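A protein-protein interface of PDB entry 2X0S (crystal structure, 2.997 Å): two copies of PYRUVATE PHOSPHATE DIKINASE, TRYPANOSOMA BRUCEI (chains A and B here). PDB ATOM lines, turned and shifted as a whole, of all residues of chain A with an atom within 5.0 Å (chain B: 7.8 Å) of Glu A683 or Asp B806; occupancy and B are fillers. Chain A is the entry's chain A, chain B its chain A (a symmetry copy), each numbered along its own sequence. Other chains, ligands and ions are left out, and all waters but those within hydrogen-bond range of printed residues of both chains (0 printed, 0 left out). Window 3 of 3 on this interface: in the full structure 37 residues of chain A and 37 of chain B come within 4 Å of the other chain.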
ATOM      1  N   PRO A 648     -26.029   4.955  18.182  1.00  0.00           N
ATOM      2  CA  PRO A 648     -26.802   6.154  18.525  1.00  0.00           C
ATOM      3  C   PRO A 648     -26.588   7.268  17.515  1.00  0.00           C
ATOM      4  O   PRO A 648     -25.552   7.296  16.856  1.00  0.00           O
ATOM      5  CB  PRO A 648     -26.195   6.595  19.865  1.00  0.00           C
ATOM      6  CG  PRO A 648     -25.281   5.496  20.282  1.00  0.00           C
ATOM      7  CD  PRO A 648     -24.835   4.850  19.033  1.00  0.00           C
ATOM      8  N   LEU A 681     -28.883  14.694  22.545  1.00  0.00           N
ATOM      9  CA  LEU A 681     -28.701  13.292  22.198  1.00  0.00           C
ATOM     10  C   LEU A 681     -27.399  12.745  22.768  1.00  0.00           C
ATOM     11  O   LEU A 681     -27.029  11.601  22.519  1.00  0.00           O
ATOM     12  CB  LEU A 681     -28.761  13.098  20.679  1.00  0.00           C
ATOM     13  CG  LEU A 681     -30.095  13.506  20.042  1.00  0.00           C
ATOM     14  CD1 LEU A 681     -30.515  12.536  18.956  1.00  0.00           C
ATOM     15  CD2 LEU A 681     -31.212  13.651  21.084  1.00  0.00           C
ATOM     16  N   HIS A 682     -26.717  13.567  23.551  1.00  0.00           N
ATOM     17  CA  HIS A 682     -25.495  13.154  24.210  1.00  0.00           C
ATOM     18  C   HIS A 682     -25.793  12.185  25.366  1.00  0.00           C
ATOM     19  O   HIS A 682     -26.785  12.345  26.083  1.00  0.00           O
ATOM     20  CB  HIS A 682     -24.758  14.385  24.712  1.00  0.00           C
ATOM     21  CG  HIS A 682     -23.621  14.078  25.631  1.00  0.00           C
ATOM     22  ND1 HIS A 682     -22.314  14.010  25.199  1.00  0.00           N
ATOM     23  CD2 HIS A 682     -23.594  13.837  26.962  1.00  0.00           C
ATOM     24  CE1 HIS A 682     -21.530  13.733  26.225  1.00  0.00           C
ATOM     25  NE2 HIS A 682     -22.282  13.622  27.306  1.00  0.00           N
ATOM     26  N   GLU A 683     -24.926  11.183  25.531  1.00  0.00           N
ATOM     27  CA  GLU A 683     -25.086  10.160  26.564  1.00  0.00           C
ATOM     28  C   GLU A 683     -23.837  10.022  27.436  1.00  0.00           C
ATOM     29  O   GLU A 683     -22.760  10.453  27.047  1.00  0.00           O
ATOM     30  CB  GLU A 683     -25.427   8.826  25.909  1.00  0.00           C
ATOM     31  CG  GLU A 683     -26.742   8.858  25.162  1.00  0.00           C
ATOM     32  CD  GLU A 683     -26.936   7.669  24.241  1.00  0.00           C
ATOM     33  OE1 GLU A 683     -28.100   7.392  23.877  1.00  0.00           O
ATOM     34  OE2 GLU A 683     -25.934   7.008  23.881  1.00  0.00           O
ATOM     35  N   LEU A 684     -23.986   9.428  28.618  1.00  0.00           N
ATOM     36  CA  LEU A 684     -22.872   9.265  29.552  1.00  0.00           C
ATOM     37  C   LEU A 684     -22.088   8.008  29.204  1.00  0.00           C
ATOM     38  O   LEU A 684     -20.863   8.026  29.087  1.00  0.00           O
ATOM     39  CB  LEU A 684     -23.381   9.106  30.981  1.00  0.00           C
ATOM     40  CG  LEU A 684     -23.988  10.263  31.762  1.00  0.00           C
ATOM     41  CD1 LEU A 684     -25.493  10.332  31.546  1.00  0.00           C
ATOM     42  CD2 LEU A 684     -23.673  10.067  33.232  1.00  0.00           C
ATOM     43  N   ASN A 685     -22.810   6.901  29.096  1.00  0.00           N
ATOM     44  CA  ASN A 685     -22.242   5.652  28.630  1.00  0.00           C
ATOM     45  C   ASN A 685     -22.979   5.324  27.357  1.00  0.00           C
ATOM     46  O   ASN A 685     -24.028   4.672  27.396  1.00  0.00           O
ATOM     47  CB  ASN A 685     -22.444   4.533  29.652  1.00  0.00           C
ATOM     48  CG  ASN A 685     -21.817   4.849  30.997  1.00  0.00           C
ATOM     49  OD1 ASN A 685     -20.603   4.776  31.167  1.00  0.00           O
ATOM     50  ND2 ASN A 685     -22.649   5.195  31.962  1.00  0.00           N
ATOM     51  N   PRO A 686     -22.446   5.807  26.224  1.00  0.00           N
ATOM     52  CA  PRO A 686     -23.040   5.692  24.888  1.00  0.00           C
ATOM     53  C   PRO A 686     -23.250   4.232  24.517  1.00  0.00           C
ATOM     54  O   PRO A 686     -24.229   3.920  23.837  1.00  0.00           O
ATOM     55  CB  PRO A 686     -21.970   6.294  23.974  1.00  0.00           C
ATOM     56  CG  PRO A 686     -21.098   7.102  24.861  1.00  0.00           C
ATOM     57  CD  PRO A 686     -21.115   6.433  26.189  1.00  0.00           C
ATOM     58  N   GLY A 689     -26.459   3.029  25.627  1.00  0.00           N
ATOM     59  CA  GLY A 689     -27.467   4.042  25.407  1.00  0.00           C
ATOM     60  C   GLY A 689     -28.599   3.605  24.499  1.00  0.00           C
ATOM     61  O   GLY A 689     -28.993   2.437  24.484  1.00  0.00           O
ATOM     62  N   HIS A 690     -29.120   4.565  23.741  1.00  0.00           N
ATOM     63  CA  HIS A 690     -30.249   4.345  22.848  1.00  0.00           C
ATOM     64  C   HIS A 690     -29.676   3.861  21.522  1.00  0.00           C
ATOM     65  O   HIS A 690     -29.031   4.630  20.813  1.00  0.00           O
ATOM     66  CB  HIS A 690     -31.012   5.669  22.679  1.00  0.00           C
ATOM     67  CG  HIS A 690     -32.406   5.533  22.129  1.00  0.00           C
ATOM     68  ND1 HIS A 690     -33.176   6.627  21.811  1.00  0.00           N
ATOM     69  CD2 HIS A 690     -33.159   4.442  21.851  1.00  0.00           C
ATOM     70  CE1 HIS A 690     -34.350   6.218  21.353  1.00  0.00           C
ATOM     71  NE2 HIS A 690     -34.365   4.901  21.370  1.00  0.00           N
ATOM     72  N   LEU B 684     -14.782   6.898  27.902  1.00  0.00           N
ATOM     73  CA  LEU B 684     -15.924   6.953  26.989  1.00  0.00           C
ATOM     74  C   LEU B 684     -17.169   6.432  27.691  1.00  0.00           C
ATOM     75  O   LEU B 684     -18.226   7.062  27.679  1.00  0.00           O
ATOM     76  CB  LEU B 684     -15.684   6.074  25.766  1.00  0.00           C
ATOM     77  CG  LEU B 684     -14.682   6.443  24.683  1.00  0.00           C
ATOM     78  CD1 LEU B 684     -13.307   5.871  24.999  1.00  0.00           C
ATOM     79  CD2 LEU B 684     -15.187   5.905  23.358  1.00  0.00           C
ATOM     80  N   ASN B 685     -17.043   5.238  28.256  1.00  0.00           N
ATOM     81  CA  ASN B 685     -18.085   4.663  29.084  1.00  0.00           C
ATOM     82  C   ASN B 685     -17.473   4.510  30.451  1.00  0.00           C
ATOM     83  O   ASN B 685     -16.861   3.478  30.747  1.00  0.00           O
ATOM     84  CB  ASN B 685     -18.528   3.299  28.554  1.00  0.00           C
ATOM     85  CG  ASN B 685     -19.056   3.365  27.133  1.00  0.00           C
ATOM     86  OD1 ASN B 685     -20.172   3.815  26.888  1.00  0.00           O
ATOM     87  ND2 ASN B 685     -18.252   2.909  26.191  1.00  0.00           N
ATOM     88  N   PRO B 686     -17.609   5.556  31.281  1.00  0.00           N
ATOM     89  CA  PRO B 686     -17.017   5.664  32.619  1.00  0.00           C
ATOM     90  C   PRO B 686     -17.483   4.520  33.507  1.00  0.00           C
ATOM     91  O   PRO B 686     -16.706   4.054  34.341  1.00  0.00           O
ATOM     92  CB  PRO B 686     -17.590   6.979  33.152  1.00  0.00           C
ATOM     93  CG  PRO B 686     -18.059   7.722  31.957  1.00  0.00           C
ATOM     94  CD  PRO B 686     -18.482   6.698  30.966  1.00  0.00           C
ATOM     95  N   MET B 687     -18.740   4.104  33.314  1.00  0.00           N
ATOM     96  CA  MET B 687     -19.386   3.011  34.047  1.00  0.00           C
ATOM     97  C   MET B 687     -18.537   1.751  34.085  1.00  0.00           C
ATOM     98  O   MET B 687     -18.398   1.098  35.119  1.00  0.00           O
ATOM     99  CB  MET B 687     -20.734   2.661  33.394  1.00  0.00           C
ATOM    100  CG  MET B 687     -21.547   1.625  34.190  1.00  0.00           C
ATOM    101  SD  MET B 687     -22.724   0.654  33.223  1.00  0.00           S
ATOM    102  CE  MET B 687     -23.990   1.842  32.796  1.00  0.00           C
ATOM    103  N   GLN B 797     -27.804  -3.125  34.839  1.00  0.00           N
ATOM    104  CA  GLN B 797     -27.301  -2.256  33.784  1.00  0.00           C
ATOM    105  C   GLN B 797     -26.414  -3.035  32.848  1.00  0.00           C
ATOM    106  O   GLN B 797     -26.494  -2.870  31.627  1.00  0.00           O
ATOM    107  CB  GLN B 797     -26.462  -1.137  34.379  1.00  0.00           C
ATOM    108  CG  GLN B 797     -27.197  -0.198  35.318  1.00  0.00           C
ATOM    109  CD  GLN B 797     -26.334   0.969  35.763  1.00  0.00           C
ATOM    110  OE1 GLN B 797     -26.175   1.948  35.025  1.00  0.00           O
ATOM    111  NE2 GLN B 797     -25.768   0.869  36.970  1.00  0.00           N
ATOM    112  N   PHE B 802     -28.181  -1.500  29.930  1.00  0.00           N
ATOM    113  CA  PHE B 802     -28.818  -0.192  30.153  1.00  0.00           C
ATOM    114  C   PHE B 802     -27.982   0.737  31.025  1.00  0.00           C
ATOM    115  O   PHE B 802     -27.780   0.463  32.212  1.00  0.00           O
ATOM    116  CB  PHE B 802     -30.172  -0.360  30.831  1.00  0.00           C
ATOM    117  CG  PHE B 802     -31.172  -1.136  30.025  1.00  0.00           C
ATOM    118  CD1 PHE B 802     -31.095  -1.182  28.639  1.00  0.00           C
ATOM    119  CD2 PHE B 802     -32.209  -1.811  30.661  1.00  0.00           C
ATOM    120  CE1 PHE B 802     -32.031  -1.903  27.903  1.00  0.00           C
ATOM    121  CE2 PHE B 802     -33.150  -2.526  29.934  1.00  0.00           C
ATOM    122  CZ  PHE B 802     -33.061  -2.577  28.557  1.00  0.00           C
ATOM    123  N   SER B 803     -27.510   1.835  30.428  1.00  0.00           N
ATOM    124  CA  SER B 803     -26.842   2.903  31.168  1.00  0.00           C
ATOM    125  C   SER B 803     -27.928   3.755  31.785  1.00  0.00           C
ATOM    126  O   SER B 803     -28.503   4.612  31.110  1.00  0.00           O
ATOM    127  CB  SER B 803     -25.997   3.769  30.240  1.00  0.00           C
ATOM    128  OG  SER B 803     -25.530   4.909  30.930  1.00  0.00           O
ATOM    129  N   ARG B 804     -28.220   3.514  33.058  1.00  0.00           N
ATOM    130  CA  ARG B 804     -29.488   3.976  33.601  1.00  0.00           C
ATOM    131  C   ARG B 804     -29.831   5.413  33.202  1.00  0.00           C
ATOM    132  O   ARG B 804     -30.929   5.684  32.702  1.00  0.00           O
ATOM    133  CB  ARG B 804     -29.551   3.823  35.120  1.00  0.00           C
ATOM    134  CG  ARG B 804     -30.942   4.126  35.653  1.00  0.00           C
ATOM    135  CD  ARG B 804     -31.022   4.073  37.158  1.00  0.00           C
ATOM    136  NE  ARG B 804     -32.406   4.169  37.602  1.00  0.00           N
ATOM    137  CZ  ARG B 804     -32.771   4.162  38.876  1.00  0.00           C
ATOM    138  NH1 ARG B 804     -31.838   4.069  39.815  1.00  0.00           N
ATOM    139  NH2 ARG B 804     -34.057   4.252  39.207  1.00  0.00           N
ATOM    140  N   ASP B 805     -28.886   6.324  33.418  1.00  0.00           N
ATOM    141  CA  ASP B 805     -29.138   7.741  33.210  1.00  0.00           C
ATOM    142  C   ASP B 805     -29.498   8.073  31.759  1.00  0.00           C
ATOM    143  O   ASP B 805     -29.896   9.195  31.464  1.00  0.00           O
ATOM    144  CB  ASP B 805     -27.926   8.577  33.641  1.00  0.00           C
ATOM    145  CG  ASP B 805     -27.205   8.004  34.851  1.00  0.00           C
ATOM    146  OD1 ASP B 805     -27.051   8.746  35.848  1.00  0.00           O
ATOM    147  OD2 ASP B 805     -26.781   6.825  34.794  1.00  0.00           O
ATOM    148  N   ASP B 806     -29.361   7.107  30.857  1.00  0.00           N
ATOM    149  CA  ASP B 806     -29.562   7.374  29.436  1.00  0.00           C
ATOM    150  C   ASP B 806     -30.815   6.732  28.864  1.00  0.00           C
ATOM    151  O   ASP B 806     -31.235   7.058  27.748  1.00  0.00           O
ATOM    152  CB  ASP B 806     -28.347   6.914  28.633  1.00  0.00           C
ATOM    153  CG  ASP B 806     -27.108   7.705  28.958  1.00  0.00           C
ATOM    154  OD1 ASP B 806     -27.156   8.942  28.831  1.00  0.00           O
ATOM    155  OD2 ASP B 806     -26.087   7.095  29.334  1.00  0.00           O
ATOM    156  N   ALA B 807     -31.398   5.814  29.629  1.00  0.00           N
ATOM    157  CA  ALA B 807     -32.563   5.057  29.176  1.00  0.00           C
ATOM    158  C   ALA B 807     -33.886   5.856  29.183  1.00  0.00           C
ATOM    159  O   ALA B 807     -34.971   5.277  29.042  1.00  0.00           O
ATOM    160  CB  ALA B 807     -32.695   3.768  29.985  1.00  0.00           C
ATOM    161  N   GLY B 808     -33.794   7.178  29.341  1.00  0.00           N
ATOM    162  CA  GLY B 808     -34.972   8.031  29.361  1.00  0.00           C
ATOM    163  C   GLY B 808     -35.834   7.871  28.123  1.00  0.00           C
ATOM    164  O   GLY B 808     -36.980   7.418  28.203  1.00  0.00           O
ATOM    165  N   PRO B 809     -35.271   8.232  26.960  1.00  0.00           N
ATOM    166  CA  PRO B 809     -35.910   8.210  25.638  1.00  0.00           C
ATOM    167  C   PRO B 809     -36.783   6.989  25.343  1.00  0.00           C
ATOM    168  O   PRO B 809     -37.711   7.106  24.548  1.00  0.00           O
ATOM    169  CB  PRO B 809     -34.716   8.220  24.681  1.00  0.00           C
ATOM    170  CG  PRO B 809     -33.661   8.961  25.409  1.00  0.00           C
ATOM    171  CD  PRO B 809     -33.880   8.723  26.886  1.00  0.00           C
ATOM    172  N   PHE B 810     -36.498   5.842  25.944  1.00  0.00           N
ATOM    173  CA  PHE B 810     -37.165   4.622  25.500  1.00  0.00           C
ATOM    174  C   PHE B 810     -37.761   3.776  26.619  1.00  0.00           C
ATOM    175  O   PHE B 810     -38.813   3.169  26.438  1.00  0.00           O
ATOM    176  CB  PHE B 810     -36.225   3.776  24.626  1.00  0.00           C
ATOM    177  CG  PHE B 810     -34.966   3.337  25.330  1.00  0.00           C
ATOM    178  CD1 PHE B 810     -34.817   2.037  25.763  1.00  0.00           C
ATOM    179  CD2 PHE B 810     -33.938   4.226  25.556  1.00  0.00           C
ATOM    180  CE1 PHE B 810     -33.668   1.637  26.407  1.00  0.00           C
ATOM    181  CE2 PHE B 810     -32.790   3.824  26.195  1.00  0.00           C
ATOM    182  CZ  PHE B 810     -32.657   2.532  26.625  1.00  0.00           C
ATOM    183  N   LEU B 811     -37.100   3.715  27.766  1.00  0.00           N
ATOM    184  CA  LEU B 811     -37.619   2.873  28.831  1.00  0.00           C
ATOM    185  C   LEU B 811     -39.069   3.227  29.116  1.00  0.00           C
ATOM    186  O   LEU B 811     -39.928   2.350  29.163  1.00  0.00           O
ATOM    187  CB  LEU B 811     -36.765   2.966  30.093  1.00  0.00           C
ATOM    188  CG  LEU B 811     -36.051   1.641  30.370  1.00  0.00           C
ATOM    189  CD1 LEU B 811     -35.638   1.482  31.836  1.00  0.00           C
ATOM    190  CD2 LEU B 811     -36.956   0.507  29.934  1.00  0.00           C
ATOM    191  N   ARG B 812     -39.339   4.518  29.286  1.00  0.00           N
ATOM    192  CA  ARG B 812     -40.695   4.984  29.531  1.00  0.00           C
ATOM    193  C   ARG B 812     -41.620   4.402  28.482  1.00  0.00           C
ATOM    194  O   ARG B 812     -42.754   4.020  28.768  1.00  0.00           O
ATOM    195  CB  ARG B 812     -40.743   6.502  29.460  1.00  0.00           C
ATOM    196  CG  ARG B 812     -39.663   7.176  30.265  1.00  0.00           C
ATOM    197  CD  ARG B 812     -39.209   8.429  29.554  1.00  0.00           C
ATOM    198  NE  ARG B 812     -39.054   9.557  30.462  1.00  0.00           N
ATOM    199  CZ  ARG B 812     -38.074   9.666  31.353  1.00  0.00           C
ATOM    200  NH1 ARG B 812     -37.167   8.704  31.466  1.00  0.00           N
ATOM    201  NH2 ARG B 812     -38.009  10.735  32.137  1.00  0.00           N
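The backbone carbonyl oxygen (O) of Leu A684 sits close to the backbone carbonyl oxygen (O) of Leu B684 (3.1 Å). The side-chain amide oxygen of Asn A685 sits at hydrogen-bond distance from the backbone NH of Met B687 (2.9 Å). The side-chain amide oxygen (OD1) of Asn A685 sits close to the backbone nitrogen (N) of Pro B686 (3.1 Å). The side-chain carboxylate (OD2) of Asp B806 lies within hydrogen-bond range of the backbone NH (N) of Asn A685, 3.3 Å away. N of Leu A684 is in hydrogen-bond range of OD1 of Asp B806. The side-chain amide nitrogen (ND2) of Asn A685 is in hydrogen-bond range of the side-chain hydroxyl (OG) of Ser B803 (3.1 Å). N of Pro A686 sits close to OD1 of Asn B685 (3.1 Å).
The side-chain hydroxyl (OG) of Ser B803 is in hydrogen-bond range of the side-chain carboxylate (OD2) of Asp B806, at 2.8 Å. The backbone NH (N) of His A690 lies within hydrogen-bond range of the side-chain carboxylate (OE1) of Glu A683 (3.0 Å).
Among the printed residues, pairs that only touch across the chains: Glu A683 with Asp B806 (3.3 Å), Leu A684 with Pro B686 (3.3 Å), Leu A684 with Asp B805 (3.7 Å), Asn A685 with Asn B685 (3.2 Å), Pro A686 with Leu B684 (3.3 Å), His A690 with Pro B809 (3.6 Å) and His A690 with Phe B810 (3.8 Å).
Glu A683 touches just one residue of chain B: Asp B806. Asp B806 touches just these residues of chain A: Glu A683, Leu A684 and Asn A685. Of the printed residues of chain A, Phe B810 touches His A690 (3.8 Å). Printed residues of chain A within 4 Å of Leu B684: Leu A684 and Pro A686. Of the printed residues of chain A, Asn B685 touches Asn A685 (3.2 Å) and Pro A686 (2.9 Å). Of the printed residues of chain B, His A690 touches Pro B809 (3.6 Å) and Phe B810 (3.8 Å). Of the printed residues of chain A, Pro B686 touches Leu A684 (3.3 Å) and Asn A685 (2.9 Å). Ala B807 touches none of the printed residues of chain A. The nearest residue of chain B that does not touch Glu A683 is Leu B684 (5.7 Å). The nearest printed residue of chain A that does not touch Asp B806 is His A682 (4.4 Å). The nearest printed residue of chain B that does not touch Leu A684 is Asn B685 (4.4 Å).
Printed residues of chain B that touch a printed residue of chain A: Leu B684, Asn B685, Pro B686, Met B687, Ser B803, Asp B805, Asp B806, Pro B809 and Phe B810. Hydrophobic or aromatic side chains of chain B within 4 Å of the printed part of chain A: Pro B686, Met B687, Pro B809 and Phe B810.
Leu A684 touches its own counterpart, Leu B684. Leu A684 touches Pro B686, and with the chains exchanged Pro A686 touches Leu B684. Asn A685 touches its own counterpart, Asn B685. Asn A685 touches Pro B686, and with the chains exchanged Pro A686 touches Asn B685.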
